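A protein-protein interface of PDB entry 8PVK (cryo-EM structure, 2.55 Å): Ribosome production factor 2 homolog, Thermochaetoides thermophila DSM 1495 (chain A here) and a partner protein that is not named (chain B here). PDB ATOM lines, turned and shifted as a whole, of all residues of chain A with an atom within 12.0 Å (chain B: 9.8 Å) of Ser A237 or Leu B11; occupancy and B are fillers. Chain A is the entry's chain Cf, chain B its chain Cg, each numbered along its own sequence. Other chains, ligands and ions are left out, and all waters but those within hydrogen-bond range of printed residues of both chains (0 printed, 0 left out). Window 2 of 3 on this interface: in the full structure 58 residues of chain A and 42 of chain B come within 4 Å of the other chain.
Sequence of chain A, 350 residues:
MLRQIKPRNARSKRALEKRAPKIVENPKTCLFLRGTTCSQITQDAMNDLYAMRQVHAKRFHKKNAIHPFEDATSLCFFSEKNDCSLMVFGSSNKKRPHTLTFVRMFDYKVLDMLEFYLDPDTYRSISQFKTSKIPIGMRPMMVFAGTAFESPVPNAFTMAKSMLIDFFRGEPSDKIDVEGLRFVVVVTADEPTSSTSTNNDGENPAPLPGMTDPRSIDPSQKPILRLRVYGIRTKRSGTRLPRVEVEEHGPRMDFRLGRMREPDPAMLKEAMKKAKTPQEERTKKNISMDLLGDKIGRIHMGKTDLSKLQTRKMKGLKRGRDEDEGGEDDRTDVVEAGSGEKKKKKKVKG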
ATOM      1  N   ARG A 233     -23.652   6.742 -12.647  1.00  0.00           N
ATOM      2  CA  ARG A 233     -23.174   7.829 -13.488  1.00  0.00           C
ATOM      3  C   ARG A 233     -22.370   8.778 -12.616  1.00  0.00           C
ATOM      4  O   ARG A 233     -22.827   9.172 -11.538  1.00  0.00           O
ATOM      5  CB  ARG A 233     -24.336   8.572 -14.150  1.00  0.00           C
ATOM      6  CG  ARG A 233     -25.082   7.773 -15.201  1.00  0.00           C
ATOM      7  CD  ARG A 233     -26.228   8.588 -15.775  1.00  0.00           C
ATOM      8  NE  ARG A 233     -27.305   8.760 -14.806  1.00  0.00           N
ATOM      9  CZ  ARG A 233     -27.630   9.915 -14.243  1.00  0.00           C
ATOM     10  NH1 ARG A 233     -26.976  11.030 -14.525  1.00  0.00           N
ATOM     11  NH2 ARG A 233     -28.634   9.952 -13.372  1.00  0.00           N
ATOM     12  N   THR A 234     -21.177   9.140 -13.071  1.00  0.00           N
ATOM     13  CA  THR A 234     -20.272   9.967 -12.289  1.00  0.00           C
ATOM     14  C   THR A 234     -19.997  11.279 -13.017  1.00  0.00           C
ATOM     15  O   THR A 234     -19.878  11.311 -14.247  1.00  0.00           O
ATOM     16  CB  THR A 234     -18.978   9.193 -11.964  1.00  0.00           C
ATOM     17  OG1 THR A 234     -18.151   9.967 -11.090  1.00  0.00           O
ATOM     18  CG2 THR A 234     -18.211   8.795 -13.216  1.00  0.00           C
ATOM     19  N   LYS A 235     -19.947  12.369 -12.251  1.00  0.00           N
ATOM     20  CA  LYS A 235     -19.887  13.723 -12.789  1.00  0.00           C
ATOM     21  C   LYS A 235     -18.777  14.511 -12.102  1.00  0.00           C
ATOM     22  O   LYS A 235     -18.215  14.088 -11.090  1.00  0.00           O
ATOM     23  CB  LYS A 235     -21.222  14.461 -12.610  1.00  0.00           C
ATOM     24  CG  LYS A 235     -22.426  13.774 -13.229  1.00  0.00           C
ATOM     25  CD  LYS A 235     -23.691  14.583 -13.000  1.00  0.00           C
ATOM     26  CE  LYS A 235     -24.904  13.904 -13.614  1.00  0.00           C
ATOM     27  NZ  LYS A 235     -26.154  14.673 -13.362  1.00  0.00           N
ATOM     28  N   ARG A 236     -18.470  15.676 -12.672  1.00  0.00           N
ATOM     29  CA  ARG A 236     -17.520  16.594 -12.058  1.00  0.00           C
ATOM     30  C   ARG A 236     -18.135  17.281 -10.844  1.00  0.00           C
ATOM     31  O   ARG A 236     -19.350  17.475 -10.757  1.00  0.00           O
ATOM     32  CB  ARG A 236     -17.058  17.650 -13.067  1.00  0.00           C
ATOM     33  CG  ARG A 236     -16.436  17.079 -14.324  1.00  0.00           C
ATOM     34  CD  ARG A 236     -15.834  18.147 -15.218  1.00  0.00           C
ATOM     35  NE  ARG A 236     -15.244  17.564 -16.417  1.00  0.00           N
ATOM     36  CZ  ARG A 236     -14.008  17.090 -16.487  1.00  0.00           C
ATOM     37  NH1 ARG A 236     -13.200  17.110 -15.439  1.00  0.00           N
ATOM     38  NH2 ARG A 236     -13.570  16.580 -17.635  1.00  0.00           N
ATOM     39  N   SER A 237     -17.276  17.649  -9.892  1.00  0.00           N
ATOM     40  CA  SER A 237     -17.704  18.392  -8.717  1.00  0.00           C
ATOM     41  C   SER A 237     -16.717  19.467  -8.281  1.00  0.00           C
ATOM     42  O   SER A 237     -16.922  20.076  -7.226  1.00  0.00           O
ATOM     43  CB  SER A 237     -17.960  17.440  -7.541  1.00  0.00           C
ATOM     44  OG  SER A 237     -16.741  16.941  -7.026  1.00  0.00           O
ATOM     45  N   GLY A 238     -15.660  19.717  -9.052  1.00  0.00           N
ATOM     46  CA  GLY A 238     -14.694  20.750  -8.739  1.00  0.00           C
ATOM     47  C   GLY A 238     -13.575  20.345  -7.804  1.00  0.00           C
ATOM     48  O   GLY A 238     -12.675  21.159  -7.558  1.00  0.00           O
ATOM     49  N   THR A 239     -13.597  19.125  -7.276  1.00  0.00           N
ATOM     50  CA  THR A 239     -12.534  18.588  -6.435  1.00  0.00           C
ATOM     51  C   THR A 239     -12.046  17.262  -7.025  1.00  0.00           C
ATOM     52  O   THR A 239     -12.451  16.860  -8.121  1.00  0.00           O
ATOM     53  CB  THR A 239     -13.018  18.434  -4.990  1.00  0.00           C
ATOM     54  OG1 THR A 239     -11.919  18.067  -4.145  1.00  0.00           O
ATOM     55  CG2 THR A 239     -14.100  17.373  -4.898  1.00  0.00           C
ATOM     56  N   ARG A 240     -11.157  16.587  -6.292  1.00  0.00           N
ATOM     57  CA  ARG A 240     -10.568  15.348  -6.790  1.00  0.00           C
ATOM     58  C   ARG A 240     -11.603  14.232  -6.861  1.00  0.00           C
ATOM     59  O   ARG A 240     -11.693  13.516  -7.864  1.00  0.00           O
ATOM     60  CB  ARG A 240      -9.393  14.933  -5.905  1.00  0.00           C
ATOM     61  CG  ARG A 240      -8.322  14.103  -6.607  1.00  0.00           C
ATOM     62  CD  ARG A 240      -8.030  14.622  -8.006  1.00  0.00           C
ATOM     63  NE  ARG A 240      -6.890  13.945  -8.612  1.00  0.00           N
ATOM     64  CZ  ARG A 240      -6.737  13.755  -9.915  1.00  0.00           C
ATOM     65  NH1 ARG A 240      -7.638  14.181 -10.785  1.00  0.00           N
ATOM     66  NH2 ARG A 240      -5.651  13.128 -10.356  1.00  0.00           N
ATOM     67  N   LEU A 241     -12.398  14.070  -5.803  1.00  0.00           N
ATOM     68  CA  LEU A 241     -13.422  13.035  -5.791  1.00  0.00           C
ATOM     69  C   LEU A 241     -14.598  13.442  -6.676  1.00  0.00           C
ATOM     70  O   LEU A 241     -14.990  14.612  -6.688  1.00  0.00           O
ATOM     71  CB  LEU A 241     -13.908  12.777  -4.369  1.00  0.00           C
ATOM     72  CG  LEU A 241     -12.811  12.464  -3.353  1.00  0.00           C
ATOM     73  CD1 LEU A 241     -13.316  12.681  -1.937  1.00  0.00           C
ATOM     74  CD2 LEU A 241     -12.307  11.039  -3.533  1.00  0.00           C
ATOM     75  N   PRO A 242     -15.169  12.507  -7.425  1.00  0.00           N
ATOM     76  CA  PRO A 242     -16.275  12.837  -8.325  1.00  0.00           C
ATOM     77  C   PRO A 242     -17.634  12.694  -7.648  1.00  0.00           C
ATOM     78  O   PRO A 242     -17.778  12.065  -6.597  1.00  0.00           O
ATOM     79  CB  PRO A 242     -16.112  11.803  -9.441  1.00  0.00           C
ATOM     80  CG  PRO A 242     -15.578  10.605  -8.735  1.00  0.00           C
ATOM     81  CD  PRO A 242     -14.693  11.125  -7.625  1.00  0.00           C
ATOM     82  N   ARG A 243     -18.639  13.290  -8.285  1.00  0.00           N
ATOM     83  CA  ARG A 243     -20.013  13.242  -7.800  1.00  0.00           C
ATOM     84  C   ARG A 243     -20.716  12.039  -8.418  1.00  0.00           C
ATOM     85  O   ARG A 243     -20.708  11.871  -9.641  1.00  0.00           O
ATOM     86  CB  ARG A 243     -20.749  14.537  -8.140  1.00  0.00           C
ATOM     87  CG  ARG A 243     -22.264  14.439  -8.075  1.00  0.00           C
ATOM     88  CD  ARG A 243     -22.786  14.726  -6.676  1.00  0.00           C
ATOM     89  NE  ARG A 243     -24.211  14.444  -6.562  1.00  0.00           N
ATOM     90  CZ  ARG A 243     -24.945  14.713  -5.491  1.00  0.00           C
ATOM     91  NH1 ARG A 243     -24.419  15.274  -4.415  1.00  0.00           N
ATOM     92  NH2 ARG A 243     -26.241  14.415  -5.501  1.00  0.00           N
ATOM     93  N   VAL A 244     -21.327  11.212  -7.575  1.00  0.00           N
ATOM     94  CA  VAL A 244     -21.922   9.946  -7.991  1.00  0.00           C
ATOM     95  C   VAL A 244     -23.427  10.125  -8.127  1.00  0.00           C
ATOM     96  O   VAL A 244     -24.084  10.634  -7.212  1.00  0.00           O
ATOM     97  CB  VAL A 244     -21.589   8.828  -6.988  1.00  0.00           C
ATOM     98  CG1 VAL A 244     -22.330   7.548  -7.335  1.00  0.00           C
ATOM     99  CG2 VAL A 244     -20.090   8.584  -6.947  1.00  0.00           C
ATOM    100  N   GLU A 245     -23.972   9.716  -9.272  1.00  0.00           N
ATOM    101  CA  GLU A 245     -25.408   9.681  -9.502  1.00  0.00           C
ATOM    102  C   GLU A 245     -25.805   8.274  -9.929  1.00  0.00           C
ATOM    103  O   GLU A 245     -25.038   7.571 -10.591  1.00  0.00           O
ATOM    104  CB  GLU A 245     -25.837  10.697 -10.570  1.00  0.00           C
ATOM    105  CG  GLU A 245     -25.519  12.142 -10.218  1.00  0.00           C
ATOM    106  CD  GLU A 245     -26.440  12.701  -9.151  1.00  0.00           C
ATOM    107  OE1 GLU A 245     -27.577  12.199  -9.017  1.00  0.00           O
ATOM    108  OE2 GLU A 245     -26.027  13.643  -8.442  1.00  0.00           O
ATOM    109  N   VAL A 246     -27.013   7.866  -9.545  1.00  0.00           N
ATOM    110  CA  VAL A 246     -27.468   6.502  -9.772  1.00  0.00           C
ATOM    111  C   VAL A 246     -28.681   6.512 -10.693  1.00  0.00           C
ATOM    112  O   VAL A 246     -29.410   7.500 -10.803  1.00  0.00           O
ATOM    113  CB  VAL A 246     -27.797   5.775  -8.453  1.00  0.00           C
ATOM    114  CG1 VAL A 246     -26.534   5.568  -7.633  1.00  0.00           C
ATOM    115  CG2 VAL A 246     -28.831   6.554  -7.660  1.00  0.00           C
ATOM    116  N   LEU B  11     -22.457  20.521  -5.930  1.00  0.00           N
ATOM    117  CA  LEU B  11     -22.940  19.401  -5.132  1.00  0.00           C
ATOM    118  C   LEU B  11     -21.784  18.717  -4.405  1.00  0.00           C
ATOM    119  O   LEU B  11     -20.716  18.520  -4.982  1.00  0.00           O
ATOM    120  CB  LEU B  11     -23.688  18.399  -6.014  1.00  0.00           C
ATOM    121  CG  LEU B  11     -25.105  18.818  -6.412  1.00  0.00           C
ATOM    122  CD1 LEU B  11     -25.756  17.762  -7.292  1.00  0.00           C
ATOM    123  CD2 LEU B  11     -25.951  19.087  -5.177  1.00  0.00           C
ATOM    124  N   PRO B  12     -21.996  18.362  -3.140  1.00  0.00           N
ATOM    125  CA  PRO B  12     -20.906  17.795  -2.341  1.00  0.00           C
ATOM    126  C   PRO B  12     -20.606  16.354  -2.721  1.00  0.00           C
ATOM    127  O   PRO B  12     -21.391  15.671  -3.384  1.00  0.00           O
ATOM    128  CB  PRO B  12     -21.438  17.889  -0.908  1.00  0.00           C
ATOM    129  CG  PRO B  12     -22.913  17.778  -1.070  1.00  0.00           C
ATOM    130  CD  PRO B  12     -23.241  18.487  -2.360  1.00  0.00           C
ATOM    131  N   VAL B  13     -19.434  15.897  -2.284  1.00  0.00           N
ATOM    132  CA  VAL B  13     -18.999  14.519  -2.471  1.00  0.00           C
ATOM    133  C   VAL B  13     -18.803  13.807  -1.141  1.00  0.00           C
ATOM    134  O   VAL B  13     -18.218  12.718  -1.104  1.00  0.00           O
ATOM    135  CB  VAL B  13     -17.719  14.449  -3.320  1.00  0.00           C
ATOM    136  CG1 VAL B  13     -18.007  14.888  -4.744  1.00  0.00           C
ATOM    137  CG2 VAL B  13     -16.626  15.306  -2.701  1.00  0.00           C
ATOM    138  N   THR B  14     -19.276  14.392  -0.046  1.00  0.00           N
ATOM    139  CA  THR B  14     -19.129  13.826   1.286  1.00  0.00           C
ATOM    140  C   THR B  14     -20.506  13.649   1.912  1.00  0.00           C
ATOM    141  O   THR B  14     -21.325  14.573   1.903  1.00  0.00           O
ATOM    142  CB  THR B  14     -18.254  14.726   2.171  1.00  0.00           C
ATOM    143  OG1 THR B  14     -16.965  14.884   1.564  1.00  0.00           O
ATOM    144  CG2 THR B  14     -18.078  14.120   3.556  1.00  0.00           C
ATOM    145  N   VAL B  15     -20.756  12.458   2.452  1.00  0.00           N
ATOM    146  CA  VAL B  15     -22.027  12.120   3.080  1.00  0.00           C
ATOM    147  C   VAL B  15     -21.812  12.046   4.584  1.00  0.00           C
ATOM    148  O   VAL B  15     -20.937  11.310   5.057  1.00  0.00           O
ATOM    149  CB  VAL B  15     -22.589  10.795   2.536  1.00  0.00           C
ATOM    150  CG1 VAL B  15     -23.862  10.411   3.274  1.00  0.00           C
ATOM    151  CG2 VAL B  15     -22.843  10.901   1.041  1.00  0.00           C
ATOM    152  N   ARG B  56     -27.443   6.293  -3.532  1.00  0.00           N
ATOM    153  CA  ARG B  56     -26.486   7.293  -3.988  1.00  0.00           C
ATOM    154  C   ARG B  56     -25.461   7.604  -2.912  1.00  0.00           C
ATOM    155  O   ARG B  56     -24.262   7.699  -3.199  1.00  0.00           O
ATOM    156  CB  ARG B  56     -27.227   8.567  -4.390  1.00  0.00           C
ATOM    157  CG  ARG B  56     -26.612   9.320  -5.544  1.00  0.00           C
ATOM    158  CD  ARG B  56     -26.726  10.821  -5.313  1.00  0.00           C
ATOM    159  NE  ARG B  56     -26.128  11.240  -4.049  1.00  0.00           N
ATOM    160  CZ  ARG B  56     -24.825  11.280  -3.794  1.00  0.00           C
ATOM    161  NH1 ARG B  56     -23.927  10.991  -4.721  1.00  0.00           N
ATOM    162  NH2 ARG B  56     -24.414  11.639  -2.582  1.00  0.00           N
ATOM    163  N   GLN B  60     -21.551   6.690  -3.304  1.00  0.00           N
ATOM    164  CA  GLN B  60     -20.595   7.790  -3.241  1.00  0.00           C
ATOM    165  C   GLN B  60     -19.531   7.545  -2.178  1.00  0.00           C
ATOM    166  O   GLN B  60     -18.338   7.757  -2.428  1.00  0.00           O
ATOM    167  CB  GLN B  60     -21.329   9.104  -2.973  1.00  0.00           C
ATOM    168  CG  GLN B  60     -20.415  10.293  -2.738  1.00  0.00           C
ATOM    169  CD  GLN B  60     -19.940  10.925  -4.029  1.00  0.00           C
ATOM    170  OE1 GLN B  60     -20.743  11.349  -4.858  1.00  0.00           O
ATOM    171  NE2 GLN B  60     -18.626  10.994  -4.205  1.00  0.00           N
ATOM    172  N   ASN B  64     -15.542   6.974  -2.886  1.00  0.00           N
ATOM    173  CA  ASN B  64     -14.531   7.785  -2.211  1.00  0.00           C
ATOM    174  C   ASN B  64     -13.542   6.919  -1.438  1.00  0.00           C
ATOM    175  O   ASN B  64     -12.331   7.171  -1.469  1.00  0.00           O
ATOM    176  CB  ASN B  64     -15.199   8.791  -1.276  1.00  0.00           C
ATOM    177  CG  ASN B  64     -16.040   9.807  -2.018  1.00  0.00           C
ATOM    178  OD1 ASN B  64     -15.874  10.008  -3.220  1.00  0.00           O
ATOM    179  ND2 ASN B  64     -16.952  10.455  -1.303  1.00  0.00           N
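Ser A237 touches just these residues of chain B: Leu B11 (3.9 Å) and Val B13 (3.3 Å).
No residue of chain B comes within 4 Å of Gly A238.
Thr A239 touches just one residue of chain B: Val B13.
Of the printed residues of chain B, Pro A242 touches Val B13 (3.4 Å) and Gln B60 (2.8 Å).
Printed residues of chain B within 4 Å of Arg A243: Leu B11 (3.6 Å), Pro B12 (3.2 Å), Val B13 (3.9 Å), Arg B56 (3.5 Å) and Gln B60 (3.6 Å).
Of the printed residues of chain B, Val A244 touches Arg B56 and Gln B60.
Leu B11 touches two residues of chain A.
Pro B12 touches just one residue of chain A: Arg A243.
Val B13 touches five residues of chain A.
Of the printed residues of chain A, Gln B60 touches Pro A242 (2.8 Å), Arg A243 (3.6 Å) and Val A244 (2.8 Å).
Of the printed residues of chain A, Asn B64 touches Leu A241 (3.6 Å).
The nearest residue of chain A that does not touch Leu B11 is Glu A245 (4.3 Å).
O of Pro A242 sits at hydrogen-bond distance from NE2 of Gln B60.
The guanidinium group of Arg A243 sits at hydrogen-bond distance from the backbone carbonyl oxygen of Pro B12 (3.2 Å).
The guanidinium group (NH1) of Arg B56 sits at hydrogen-bond distance from the backbone carbonyl oxygen (O) of Val A244.
The backbone NH of Val A244 lies within hydrogen-bond range of the side-chain amide oxygen of Gln B60, 2.8 Å away.
NH2 of Arg A243 lies close to NE of Arg B56 (3.5 Å).
Of the 8 printed residues of chain B, 6 touch a printed residue of chain A.
Hydrophobic or aromatic side chains of chain A that line the printed part of chain B: Leu A241 and Val A244.
The backbone carbonyl oxygen (O) of Arg A243 is in hydrogen-bond range of the backbone NH (N) of Lys A235, at 2.8 Å.
The side-chain hydroxyl of Ser A237 is in hydrogen-bond range of the backbone carbonyl oxygen of Leu A241.
The side-chain carboxylate (OE2) of Glu A245 lies within salt-bridge range of the guanidinium group (NE) of Arg A243 (2.7 Å).
The backbone carbonyl oxygen (O) of Val B13 lies within hydrogen-bond range of the side-chain amide nitrogen (ND2) of Asn B64 (2.6 Å).
OE1 of Gln B60 lies within hydrogen-bond range of NH1 of Arg B56.
The side-chain amide nitrogen (NE2) of Gln B60 is in hydrogen-bond range of the side-chain amide oxygen (OD1) of Asn B64 (3.1 Å).
Among the printed residues, merely in contact across the chains: Ser A237 with Leu B11, Ser A237 with Val B13, Thr A239 with Val B13, Leu A241 with Val B13, Leu A241 with Asn B64, Pro A242 with Val B13, Arg A243 with Leu B11, Arg A243 with Val B13 and Arg A243 with Gln B60.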
